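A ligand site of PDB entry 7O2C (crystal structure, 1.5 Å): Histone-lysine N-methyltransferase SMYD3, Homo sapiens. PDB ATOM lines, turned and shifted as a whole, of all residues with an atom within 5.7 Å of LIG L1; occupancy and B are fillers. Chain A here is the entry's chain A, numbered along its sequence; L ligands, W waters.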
ATOM      1  N   ASN A  13      37.752  33.895  28.738  1.00  0.00           N
ATOM      2  CA  ASN A  13      36.945  34.240  29.939  1.00  0.00           C
ATOM      3  C   ASN A  13      35.659  33.448  30.078  1.00  0.00           C
ATOM      4  O   ASN A  13      34.789  33.838  30.875  1.00  0.00           O
ATOM      5  CB  ASN A  13      36.621  35.737  29.972  1.00  0.00           C
ATOM      6  CG  ASN A  13      35.815  36.267  28.806  1.00  0.00           C
ATOM      7  OD1 ASN A  13      35.025  35.560  28.184  1.00  0.00           O
ATOM      8  ND2 ASN A  13      36.026  37.533  28.503  1.00  0.00           N
ATOM      9  N   ARG A  14      35.520  32.324  29.362  1.00  0.00           N
ATOM     10  CA  ARG A  14      34.335  31.509  29.600  1.00  0.00           C
ATOM     11  C   ARG A  14      34.710  30.053  29.616  1.00  0.00           C
ATOM     12  O   ARG A  14      33.928  29.246  29.240  1.00  0.00           O
ATOM     13  CB  ARG A  14      33.233  31.894  28.647  1.00  0.00           C
ATOM     14  CG  ARG A  14      33.675  31.935  27.214  1.00  0.00           C
ATOM     15  CD  ARG A  14      32.992  33.208  26.844  1.00  0.00           C
ATOM     16  NE  ARG A  14      32.571  33.066  25.499  1.00  0.00           N
ATOM     17  CZ  ARG A  14      31.871  33.959  24.861  1.00  0.00           C
ATOM     18  NH1 ARG A  14      31.514  35.078  25.475  1.00  0.00           N
ATOM     19  NH2 ARG A  14      31.553  33.731  23.602  1.00  0.00           N
ATOM     20  N   GLY A  15      35.859  29.727  30.184  1.00  0.00           N
ATOM     21  CA  GLY A  15      36.225  28.345  30.330  1.00  0.00           C
ATOM     22  C   GLY A  15      36.551  27.730  29.019  1.00  0.00           C
ATOM     23  O   GLY A  15      37.156  28.399  28.180  1.00  0.00           O
ATOM     24  N   ASN A  16      36.298  26.443  28.954  1.00  0.00           N
ATOM     25  CA  ASN A  16      36.525  25.688  27.706  1.00  0.00           C
ATOM     26  C   ASN A  16      35.397  26.028  26.723  1.00  0.00           C
ATOM     27  O   ASN A  16      34.282  26.348  27.142  1.00  0.00           O
ATOM     28  CB  ASN A  16      36.653  24.188  27.958  1.00  0.00           C
ATOM     29  CG  ASN A  16      37.812  23.893  28.881  1.00  0.00           C
ATOM     30  OD1 ASN A  16      37.642  23.106  29.820  1.00  0.00           O
ATOM     31  ND2 ASN A  16      38.935  24.523  28.566  1.00  0.00           N
ATOM     32  N   GLY A  17      35.713  25.920  25.424  1.00  0.00           N
ATOM     33  CA  GLY A  17      34.657  26.062  24.401  1.00  0.00           C
ATOM     34  C   GLY A  17      35.035  25.238  23.192  1.00  0.00           C
ATOM     35  O   GLY A  17      36.037  24.513  23.176  1.00  0.00           O
ATOM     36  N   TYR A 124      35.080  15.637  25.279  1.00  0.00           N
ATOM     37  CA  TYR A 124      34.925  16.148  26.651  1.00  0.00           C
ATOM     38  C   TYR A 124      34.050  15.165  27.397  1.00  0.00           C
ATOM     39  O   TYR A 124      33.094  14.631  26.847  1.00  0.00           O
ATOM     40  CB  TYR A 124      34.215  17.485  26.613  1.00  0.00           C
ATOM     41  CG  TYR A 124      34.454  18.507  27.719  1.00  0.00           C
ATOM     42  CD1 TYR A 124      35.732  18.929  28.054  1.00  0.00           C
ATOM     43  CD2 TYR A 124      33.409  19.220  28.255  1.00  0.00           C
ATOM     44  CE1 TYR A 124      35.938  19.977  28.934  1.00  0.00           C
ATOM     45  CE2 TYR A 124      33.584  20.249  29.171  1.00  0.00           C
ATOM     46  CZ  TYR A 124      34.872  20.676  29.436  1.00  0.00           C
ATOM     47  OH  TYR A 124      35.069  21.761  30.247  1.00  0.00           O
ATOM     48  N   ASP A 128      35.147  15.983  33.064  1.00  0.00           N
ATOM     49  CA  ASP A 128      35.635  17.302  32.653  1.00  0.00           C
ATOM     50  C   ASP A 128      34.582  18.408  32.789  1.00  0.00           C
ATOM     51  O   ASP A 128      34.994  19.581  32.712  1.00  0.00           O
ATOM     52  CB  ASP A 128      36.037  17.280  31.189  1.00  0.00           C
ATOM     53  CG  ASP A 128      37.142  16.325  30.799  1.00  0.00           C
ATOM     54  OD1 ASP A 128      38.114  16.118  31.597  1.00  0.00           O
ATOM     55  OD2 ASP A 128      37.015  15.766  29.639  1.00  0.00           O
ATOM     56  N   LEU A 129      33.280  18.100  32.933  1.00  0.00           N
ATOM     57  CA  LEU A 129      32.281  19.159  32.817  1.00  0.00           C
ATOM     58  C   LEU A 129      32.482  20.264  33.850  1.00  0.00           C
ATOM     59  O   LEU A 129      32.886  19.982  35.026  1.00  0.00           O
ATOM     60  CB  LEU A 129      30.855  18.632  32.933  1.00  0.00           C
ATOM     61  CG  LEU A 129      30.441  17.602  31.871  1.00  0.00           C
ATOM     62  CD1 LEU A 129      29.104  16.987  32.272  1.00  0.00           C
ATOM     63  CD2 LEU A 129      30.343  18.315  30.545  1.00  0.00           C
ATOM     64  N   GLU A 130      32.109  21.468  33.462  1.00  0.00           N
ATOM     65  CA  GLU A 130      32.034  22.668  34.338  1.00  0.00           C
ATOM     66  C   GLU A 130      30.998  22.401  35.445  1.00  0.00           C
ATOM     67  O   GLU A 130      29.869  22.002  35.173  1.00  0.00           O
ATOM     68  CB  GLU A 130      31.659  23.961  33.587  1.00  0.00           C
ATOM     69  CG  GLU A 130      31.553  25.195  34.486  1.00  0.00           C
ATOM     70  CD  GLU A 130      32.887  25.568  35.042  1.00  0.00           C
ATOM     71  OE1 GLU A 130      33.739  26.001  34.283  1.00  0.00           O
ATOM     72  OE2 GLU A 130      33.058  25.304  36.256  1.00  0.00           O
ATOM     73  N   ASN A 132      30.939  25.016  38.163  1.00  0.00           N
ATOM     74  CA  ASN A 132      30.764  26.360  38.763  1.00  0.00           C
ATOM     75  C   ASN A 132      30.665  26.293  40.276  1.00  0.00           C
ATOM     76  O   ASN A 132      30.059  27.192  40.830  1.00  0.00           O
ATOM     77  CB  ASN A 132      29.487  27.061  38.235  1.00  0.00           C
ATOM     78  CG  ASN A 132      29.654  27.441  36.778  1.00  0.00           C
ATOM     79  OD1 ASN A 132      30.663  27.992  36.387  1.00  0.00           O
ATOM     80  ND2 ASN A 132      28.771  26.988  35.935  1.00  0.00           N
ATOM     81  N   LYS A 135      31.098  29.509  42.303  1.00  0.00           N
ATOM     82  CA  LYS A 135      30.114  30.606  42.151  1.00  0.00           C
ATOM     83  C   LYS A 135      28.749  30.237  42.718  1.00  0.00           C
ATOM     84  O   LYS A 135      27.872  31.122  42.726  1.00  0.00           O
ATOM     85  CB  LYS A 135      29.955  30.905  40.664  1.00  0.00           C
ATOM     86  CG  LYS A 135      31.231  31.490  40.035  1.00  0.00           C
ATOM     87  CD  LYS A 135      31.103  31.622  38.541  1.00  0.00           C
ATOM     88  CE  LYS A 135      32.253  32.378  37.904  1.00  0.00           C
ATOM     89  NZ  LYS A 135      31.928  32.798  36.503  1.00  0.00           N
ATOM     90  N   CYS A 180      24.179  22.782  34.981  1.00  0.00           N
ATOM     91  CA  CYS A 180      24.669  23.721  33.974  1.00  0.00           C
ATOM     92  C   CYS A 180      25.096  22.994  32.676  1.00  0.00           C
ATOM     93  O   CYS A 180      25.549  23.708  31.801  1.00  0.00           O
ATOM     94  CB  CYS A 180      25.747  24.671  34.451  1.00  0.00           C
ATOM     95  SG  CYS A 180      27.299  23.832  34.824  1.00  0.00           S
ATOM     96  N   ASN A 181      24.857  21.689  32.550  1.00  0.00           N
ATOM     97  CA  ASN A 181      25.151  20.901  31.328  1.00  0.00           C
ATOM     98  C   ASN A 181      23.965  20.065  30.806  1.00  0.00           C
ATOM     99  O   ASN A 181      24.157  19.410  29.821  1.00  0.00           O
ATOM    100  CB  ASN A 181      26.386  20.067  31.502  1.00  0.00           C
ATOM    101  CG  ASN A 181      27.625  20.939  31.747  1.00  0.00           C
ATOM    102  OD1 ASN A 181      28.206  21.465  30.802  1.00  0.00           O
ATOM    103  ND2 ASN A 181      28.078  21.035  33.006  1.00  0.00           N
ATOM    104  N   SER A 202      28.604  19.761  25.339  1.00  0.00           N
ATOM    105  CA  SER A 202      28.572  20.668  26.487  1.00  0.00           C
ATOM    106  C   SER A 202      29.734  21.655  26.438  1.00  0.00           C
ATOM    107  O   SER A 202      29.734  22.589  27.250  1.00  0.00           O
ATOM    108  CB  SER A 202      28.721  19.856  27.764  1.00  0.00           C
ATOM    109  OG  SER A 202      27.667  19.011  28.055  1.00  0.00           O
ATOM    110  N   LEU A 203      30.697  21.457  25.555  1.00  0.00           N
ATOM    111  CA  LEU A 203      31.749  22.476  25.325  1.00  0.00           C
ATOM    112  C   LEU A 203      31.164  23.805  24.819  1.00  0.00           C
ATOM    113  O   LEU A 203      31.809  24.851  25.007  1.00  0.00           O
ATOM    114  CB  LEU A 203      32.828  21.957  24.410  1.00  0.00           C
ATOM    115  CG  LEU A 203      33.836  21.033  25.068  1.00  0.00           C
ATOM    116  CD1 LEU A 203      34.642  20.348  23.986  1.00  0.00           C
ATOM    117  CD2 LEU A 203      34.719  21.851  26.019  1.00  0.00           C
ATOM    118  N   LEU A 204      29.991  23.776  24.200  1.00  0.00           N
ATOM    119  CA  LEU A 204      29.472  25.009  23.546  1.00  0.00           C
ATOM    120  C   LEU A 204      29.066  26.027  24.585  1.00  0.00           C
ATOM    121  O   LEU A 204      28.235  25.700  25.502  1.00  0.00           O
ATOM    122  CB  LEU A 204      28.220  24.677  22.727  1.00  0.00           C
ATOM    123  CG  LEU A 204      28.468  23.800  21.491  1.00  0.00           C
ATOM    124  CD1 LEU A 204      27.157  23.086  21.110  1.00  0.00           C
ATOM    125  CD2 LEU A 204      28.999  24.650  20.354  1.00  0.00           C
ATOM    126  N   ASN A 205      29.661  27.199  24.483  1.00  0.00           N
ATOM    127  CA  ASN A 205      29.213  28.366  25.240  1.00  0.00           C
ATOM    128  C   ASN A 205      27.973  29.030  24.623  1.00  0.00           C
ATOM    129  O   ASN A 205      27.571  28.731  23.478  1.00  0.00           O
ATOM    130  CB  ASN A 205      30.390  29.329  25.430  1.00  0.00           C
ATOM    131  CG  ASN A 205      31.397  28.702  26.396  1.00  0.00           C
ATOM    132  OD1 ASN A 205      30.975  28.243  27.470  1.00  0.00           O
ATOM    133  ND2 ASN A 205      32.667  28.784  26.004  1.00  0.00           N
ATOM    134  N   HIS A 206      27.335  29.822  25.415  1.00  0.00           N
ATOM    135  CA  HIS A 206      26.033  30.492  25.119  1.00  0.00           C
ATOM    136  C   HIS A 206      26.250  31.813  24.399  1.00  0.00           C
ATOM    137  O   HIS A 206      27.148  32.571  24.726  1.00  0.00           O
ATOM    138  CB  HIS A 206      25.299  30.781  26.417  1.00  0.00           C
ATOM    139  CG  HIS A 206      24.215  31.787  26.239  1.00  0.00           C
ATOM    140  ND1 HIS A 206      22.943  31.359  25.801  1.00  0.00           N
ATOM    141  CD2 HIS A 206      24.161  33.111  26.398  1.00  0.00           C
ATOM    142  CE1 HIS A 206      22.210  32.468  25.684  1.00  0.00           C
ATOM    143  NE2 HIS A 206      22.917  33.545  26.100  1.00  0.00           N
ATOM    144  N   SER A 207      25.354  32.172  23.477  1.00  0.00           N
ATOM    145  CA  SER A 207      25.198  33.508  22.900  1.00  0.00           C
ATOM    146  C   SER A 207      23.702  33.747  22.768  1.00  0.00           C
ATOM    147  O   SER A 207      22.985  32.837  22.445  1.00  0.00           O
ATOM    148  CB  SER A 207      25.890  33.680  21.539  1.00  0.00           C
ATOM    149  OG  SER A 207      25.556  34.937  20.996  1.00  0.00           O
ATOM    150  N   TYR A 239      21.395  29.059  24.872  1.00  0.00           N
ATOM    151  CA  TYR A 239      20.930  28.055  25.861  1.00  0.00           C
ATOM    152  C   TYR A 239      19.418  28.181  26.131  1.00  0.00           C
ATOM    153  O   TYR A 239      18.854  27.256  26.732  1.00  0.00           O
ATOM    154  CB  TYR A 239      21.676  28.195  27.199  1.00  0.00           C
ATOM    155  CG  TYR A 239      23.144  27.885  27.228  1.00  0.00           C
ATOM    156  CD1 TYR A 239      23.857  27.384  26.150  1.00  0.00           C
ATOM    157  CD2 TYR A 239      23.835  28.051  28.407  1.00  0.00           C
ATOM    158  CE1 TYR A 239      25.193  27.053  26.177  1.00  0.00           C
ATOM    159  CE2 TYR A 239      25.161  27.744  28.454  1.00  0.00           C
ATOM    160  CZ  TYR A 239      25.858  27.231  27.388  1.00  0.00           C
ATOM    161  OH  TYR A 239      27.186  26.945  27.496  1.00  0.00           O
ATOM    162  N   GLN A 256      21.178  29.483  36.859  1.00  0.00           N
ATOM    163  CA  GLN A 256      21.437  28.140  36.334  1.00  0.00           C
ATOM    164  C   GLN A 256      22.880  28.021  35.865  1.00  0.00           C
ATOM    165  O   GLN A 256      23.479  26.931  36.057  1.00  0.00           O
ATOM    166  CB  GLN A 256      20.434  27.814  35.241  1.00  0.00           C
ATOM    167  CG  GLN A 256      20.578  26.405  34.742  1.00  0.00           C
ATOM    168  CD  GLN A 256      19.510  25.950  33.787  1.00  0.00           C
ATOM    169  OE1 GLN A 256      18.584  26.710  33.483  1.00  0.00           O
ATOM    170  NE2 GLN A 256      19.687  24.718  33.335  1.00  0.00           N
ATOM    171  N   TYR A 257      23.436  29.067  35.270  1.00  0.00           N
ATOM    172  CA  TYR A 257      24.752  28.969  34.571  1.00  0.00           C
ATOM    173  C   TYR A 257      25.886  29.752  35.233  1.00  0.00           C
ATOM    174  O   TYR A 257      26.987  29.657  34.746  1.00  0.00           O
ATOM    175  CB  TYR A 257      24.556  29.334  33.086  1.00  0.00           C
ATOM    176  CG  TYR A 257      23.612  28.354  32.409  1.00  0.00           C
ATOM    177  CD1 TYR A 257      24.030  27.104  32.026  1.00  0.00           C
ATOM    178  CD2 TYR A 257      22.324  28.713  32.108  1.00  0.00           C
ATOM    179  CE1 TYR A 257      23.228  26.183  31.405  1.00  0.00           C
ATOM    180  CE2 TYR A 257      21.505  27.807  31.410  1.00  0.00           C
ATOM    181  CZ  TYR A 257      21.928  26.542  31.087  1.00  0.00           C
ATOM    182  OH  TYR A 257      21.164  25.583  30.475  1.00  0.00           O
ATOM    183  N   CYS A 258      25.567  30.561  36.223  1.00  0.00           N
ATOM    184  CA  CYS A 258      26.562  31.337  36.978  1.00  0.00           C
ATOM    185  C   CYS A 258      27.395  32.200  36.039  1.00  0.00           C
ATOM    186  O   CYS A 258      28.614  32.250  36.136  1.00  0.00           O
ATOM    187  CB  CYS A 258      27.486  30.401  37.786  1.00  0.00           C
ATOM    188  SG  CYS A 258      26.609  29.611  39.157  1.00  0.00           S
ATOM    189  N   PHE A 259      26.766  32.937  35.124  1.00  0.00           N
ATOM    190  CA  PHE A 259      27.477  33.997  34.412  1.00  0.00           C
ATOM    191  C   PHE A 259      26.582  35.152  33.991  1.00  0.00           C
ATOM    192  O   PHE A 259      25.365  35.022  34.094  1.00  0.00           O
ATOM    193  CB  PHE A 259      28.244  33.477  33.193  1.00  0.00           C
ATOM    194  CG  PHE A 259      27.399  33.151  31.983  1.00  0.00           C
ATOM    195  CD1 PHE A 259      27.210  34.113  30.972  1.00  0.00           C
ATOM    196  CD2 PHE A 259      26.823  31.899  31.858  1.00  0.00           C
ATOM    197  CE1 PHE A 259      26.389  33.765  29.893  1.00  0.00           C
ATOM    198  CE2 PHE A 259      25.984  31.580  30.805  1.00  0.00           C
ATOM    199  CZ  PHE A 259      25.834  32.500  29.790  1.00  0.00           C
ATOM    200  N   GLU A 260      27.266  36.260  33.761  1.00  0.00           N
ATOM    201  CA  GLU A 260      26.743  37.583  33.383  1.00  0.00           C
ATOM    202  C   GLU A 260      27.010  37.719  31.893  1.00  0.00           C
ATOM    203  O   GLU A 260      28.127  37.575  31.419  1.00  0.00           O
ATOM    204  CB  GLU A 260      27.511  38.675  34.141  1.00  0.00           C
ATOM    205  CG  GLU A 260      27.654  38.418  35.663  1.00  0.00           C
ATOM    206  CD  GLU A 260      26.386  38.249  36.456  1.00  0.00           C
ATOM    207  OE1 GLU A 260      25.240  38.593  35.972  1.00  0.00           O
ATOM    208  OE2 GLU A 260      26.480  37.762  37.631  1.00  0.00           O
ATOM    209  N   CYS A 261      25.984  38.093  31.132  1.00  0.00           N
ATOM    210  CA  CYS A 261      26.202  38.292  29.689  1.00  0.00           C
ATOM    211  C   CYS A 261      26.291  39.766  29.325  1.00  0.00           C
ATOM    212  O   CYS A 261      25.381  40.527  29.684  1.00  0.00           O
ATOM    213  CB  CYS A 261      25.079  37.615  28.917  1.00  0.00           C
ATOM    214  SG  CYS A 261      25.319  37.741  27.109  1.00  0.00           S
HETATM  215  N1  LIG L   1      32.615  26.836  29.362  1.00  0.00           N
HETATM  216  C1  LIG L   1      32.094  25.473  29.674  1.00  0.00           C
HETATM  217  C2  LIG L   1      33.234  24.522  30.108  1.00  0.00           C
HETATM  218  O1  LIG L   1      32.985  23.361  30.237  1.00  0.00           O
HETATM  219  O2  LIG L   1      34.322  25.081  30.382  1.00  0.00           O
HETATM  220  C3  LIG L   1      31.320  24.898  28.475  1.00  0.00           C
HETATM  221  C4  LIG L   1      29.858  25.369  28.452  1.00  0.00           C
HETATM  222  S1  LIG L   1      28.919  24.643  29.793  1.00  0.00           S
HETATM  223  C5  LIG L   1      27.486  23.925  29.054  1.00  0.00           C
HETATM  224  C6  LIG L   1      28.089  26.048  30.558  1.00  0.00           C
HETATM  225  C7  LIG L   1      28.968  26.985  31.385  1.00  0.00           C
HETATM  226  O3  LIG L   1      29.924  27.637  30.532  1.00  0.00           O
HETATM  227  C8  LIG L   1      28.263  28.109  32.110  1.00  0.00           C
HETATM  228  O4  LIG L   1      27.633  27.634  33.290  1.00  0.00           O
HETATM  229  C9  LIG L   1      29.403  29.131  32.289  1.00  0.00           C
HETATM  230  O5  LIG L   1      30.311  28.663  33.278  1.00  0.00           O
HETATM  231  C10 LIG L   1      30.117  28.984  30.942  1.00  0.00           C
HETATM  232  N2  LIG L   1      29.579  29.867  29.907  1.00  0.00           N
HETATM  233  C11 LIG L   1      28.754  29.539  28.843  1.00  0.00           C
HETATM  234  N3  LIG L   1      28.460  30.567  28.073  1.00  0.00           N
HETATM  235  C12 LIG L   1      29.111  31.640  28.631  1.00  0.00           C
HETATM  236  C13 LIG L   1      29.174  32.986  28.264  1.00  0.00           C
HETATM  237  N4  LIG L   1      28.612  33.481  27.152  1.00  0.00           N
HETATM  238  N5  LIG L   1      29.882  33.835  29.045  1.00  0.00           N
HETATM  239  C14 LIG L   1      30.476  33.298  30.145  1.00  0.00           C
HETATM  240  N6  LIG L   1      30.502  32.036  30.570  1.00  0.00           N
HETATM  241  C15 LIG L   1      29.794  31.213  29.763  1.00  0.00           C
HETATM  242  C1  LG2 L   2      15.947  24.053  23.084  1.00  0.00           C
HETATM  243  C2  LG2 L   2      16.486  25.240  23.750  1.00  0.00           C
HETATM  244  C3  LG2 L   2      17.547  24.963  24.659  1.00  0.00           C
HETATM  245  C4  LG2 L   2      15.133  24.211  20.754  1.00  0.00           C
HETATM  246  C5  LG2 L   2      15.514  21.758  21.356  1.00  0.00           C
HETATM  247  C6  LG2 L   2      15.737  25.416  20.145  1.00  0.00           C
HETATM  248  C7  LG2 L   2      22.171  23.826  26.631  1.00  0.00           C
HETATM  249  C8  LG2 L   2      24.013  24.067  28.433  1.00  0.00           C
HETATM  250  C9  LG2 L   2      13.811  25.047  22.647  1.00  0.00           C
HETATM  251  C10 LG2 L   2      11.476  24.989  25.264  1.00  0.00           C
HETATM  252  C11 LG2 L   2      13.792  24.204  24.938  1.00  0.00           C
HETATM  253  C12 LG2 L   2      12.296  25.889  24.410  1.00  0.00           C
HETATM  254  C13 LG2 L   2      11.084  23.674  24.591  1.00  0.00           C
HETATM  255  C14 LG2 L   2      12.404  23.724  25.487  1.00  0.00           C
HETATM  256  N1  LG2 L   2      13.434  25.162  23.954  1.00  0.00           N
HETATM  257  O1  LG2 L   2      13.079  25.667  21.824  1.00  0.00           O
HETATM  258  N2  LG2 L   2      14.874  24.393  22.234  1.00  0.00           N
HETATM  259  C15 LG2 L   2      15.982  22.922  20.524  1.00  0.00           C
HETATM  260  O2  LG2 L   2      14.991  20.711  21.001  1.00  0.00           O
HETATM  261  N3  LG2 L   2      15.930  21.727  22.632  1.00  0.00           N
HETATM  262  C16 LG2 L   2      16.426  22.840  23.293  1.00  0.00           C
HETATM  263  C17 LG2 L   2      17.529  22.581  24.182  1.00  0.00           C
HETATM  264  C18 LG2 L   2      18.037  23.696  24.897  1.00  0.00           C
HETATM  265  C19 LG2 L   2      19.177  23.415  25.897  1.00  0.00           C
HETATM  266  O3  LG2 L   2      19.438  22.251  26.093  1.00  0.00           O
HETATM  267  N4  LG2 L   2      19.752  24.484  26.474  1.00  0.00           N
HETATM  268  C20 LG2 L   2      20.889  24.125  27.352  1.00  0.00           C
HETATM  269  C21 LG2 L   2      23.143  23.117  27.613  1.00  0.00           C
HETATM  270  C22 LG2 L   2      24.587  23.271  27.227  1.00  0.00           C
HETATM  271  O   HOH W   1      28.212  36.395  26.421  1.00  0.00           O
HETATM  272  O   HOH W   2      29.979  36.645  29.205  1.00  0.00           O
HETATM  273  O   HOH W   3      32.950  27.714  32.048  1.00  0.00           O
HETATM  274  O   HOH W   4      31.963  32.060  32.949  1.00  0.00           O
HETATM  275  O   HOH W   5      35.590  24.491  32.679  1.00  0.00           O
HETATM  276  O   HOH W   6      30.882  21.695  30.953  1.00  0.00           O
HETATM  277  O   HOH W   7      30.550  30.824  35.092  1.00  0.00           O
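O4 of LIG L1 is in hydrogen-bond range of O of Tyr 257, 2.6 Å away. The side-chain hydroxyl (OH) of Tyr 124 sits at hydrogen-bond distance from an oxygen (O1) of LIG L1 (2.6 Å). The backbone carbonyl oxygen (O) of Arg 14 sits at hydrogen-bond distance from a nitrogen (N1) of LIG L1 (2.7 Å). The backbone NH (N) of Asn 16 lies within hydrogen-bond range of an oxygen (O2) of LIG L1 (2.8 Å). O of Asn 16 lies within hydrogen-bond range of N1 of LIG L1 (2.8 Å). A nitrogen (N1) of LIG L1 lies within hydrogen-bond range of the side-chain amide oxygen (OD1) of Asn 205, 2.9 Å away. ND2 of Asn 132 sits at hydrogen-bond distance from O4 of LIG L1, 3.0 Å away. N of His 206 sits at hydrogen-bond distance from N3 of LIG L1 (3.0 Å). O of His 206 is in hydrogen-bond range of N4 of LIG L1 (3.0 Å). O of Tyr 239 lies within hydrogen-bond range of N4 of LG2 L2, 2.9 Å away.
The side-chain amide oxygen (OD1) of Asn 181 lies close to a sulfur (S1) of LIG L1, 3.4 Å away. The backbone carbonyl oxygen of Ser 202 lies close to a sulfur (S1) of LIG L1 (3.4 Å). OH of Tyr 239 sits close to S1 of LIG L1, 3.7 Å away. Residues that only touch LIG L1: Gly 15 (3.7 Å), Glu 130 (3.7 Å), Cys 180 (3.4 Å), Leu 203 (3.5 Å), Leu 204 (3.4 Å) and Phe 259 (3.3 Å). Hydrophobic or aromatic side chains that line LIG L1: Tyr 124, His 206, Tyr 239, Tyr 257 and Phe 259. 16 residues have an atom within 4 Å of LIG L1: Arg 14, Gly 15, Asn 16, Tyr 124, Glu 130, Asn 132, Cys 180, Asn 181, Ser 202, Leu 203, Leu 204, Asn 205, His 206, Tyr 239, Tyr 257 and Phe 259.
The backbone carbonyl oxygen (O) of Tyr 257 lies within hydrogen-bond range of the side-chain amide nitrogen (ND2) of Asn 132 (3.4 Å). The side-chain hydroxyl of Tyr 124 sits at hydrogen-bond distance from the backbone carbonyl oxygen of Asp 128. O of Asn 16 is in hydrogen-bond range of ND2 of Asn 205 (3.1 Å). The side-chain amide nitrogen of Asn 132 lies within hydrogen-bond range of the side-chain sulfur of Cys 180, at 3.7 Å. The backbone NH of Tyr 239 sits at hydrogen-bond distance from a ring nitrogen (ND1) of His 206, 2.9 Å away. The side-chain amide nitrogen of Asn 181 is in hydrogen-bond range of the side-chain sulfur of Cys 180 (3.4 Å). ND2 of Asn 181 sits at hydrogen-bond distance from O of Glu 130 (3.0 Å). The backbone carbonyl oxygen (O) of Glu 130 lies within hydrogen-bond range of the side-chain sulfur (SG) of Cys 180 (3.2 Å).
Water W5 bridges an oxygen (O2) of LIG L1 (2.7 Å) and the side-chain carboxylate (OE1) of Glu 130 (2.9 Å). Water W6 lies within hydrogen-bond range of OD1 of Asn 181 (2.7 Å), O1 of LIG L1 (2.8 Å) and N of Glu 130 (2.8 Å). Water W2 lies within hydrogen-bond range of N5 of LIG L1 (2.8 Å) and O of Glu 260 (3.0 Å). Water W7 lies within hydrogen-bond range of O of Cys 258 (2.6 Å), NZ of Lys 135 (2.8 Å), O5 of LIG L1 (2.8 Å) and OD1 of Asn 132 (3.1 Å). Water W3 lies within hydrogen-bond range of a nitrogen (N1) of LIG L1 (2.8 Å), the side-chain carboxylate of Glu 130 (2.9 Å) and the backbone carbonyl oxygen of Arg 14 (3.3 Å).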
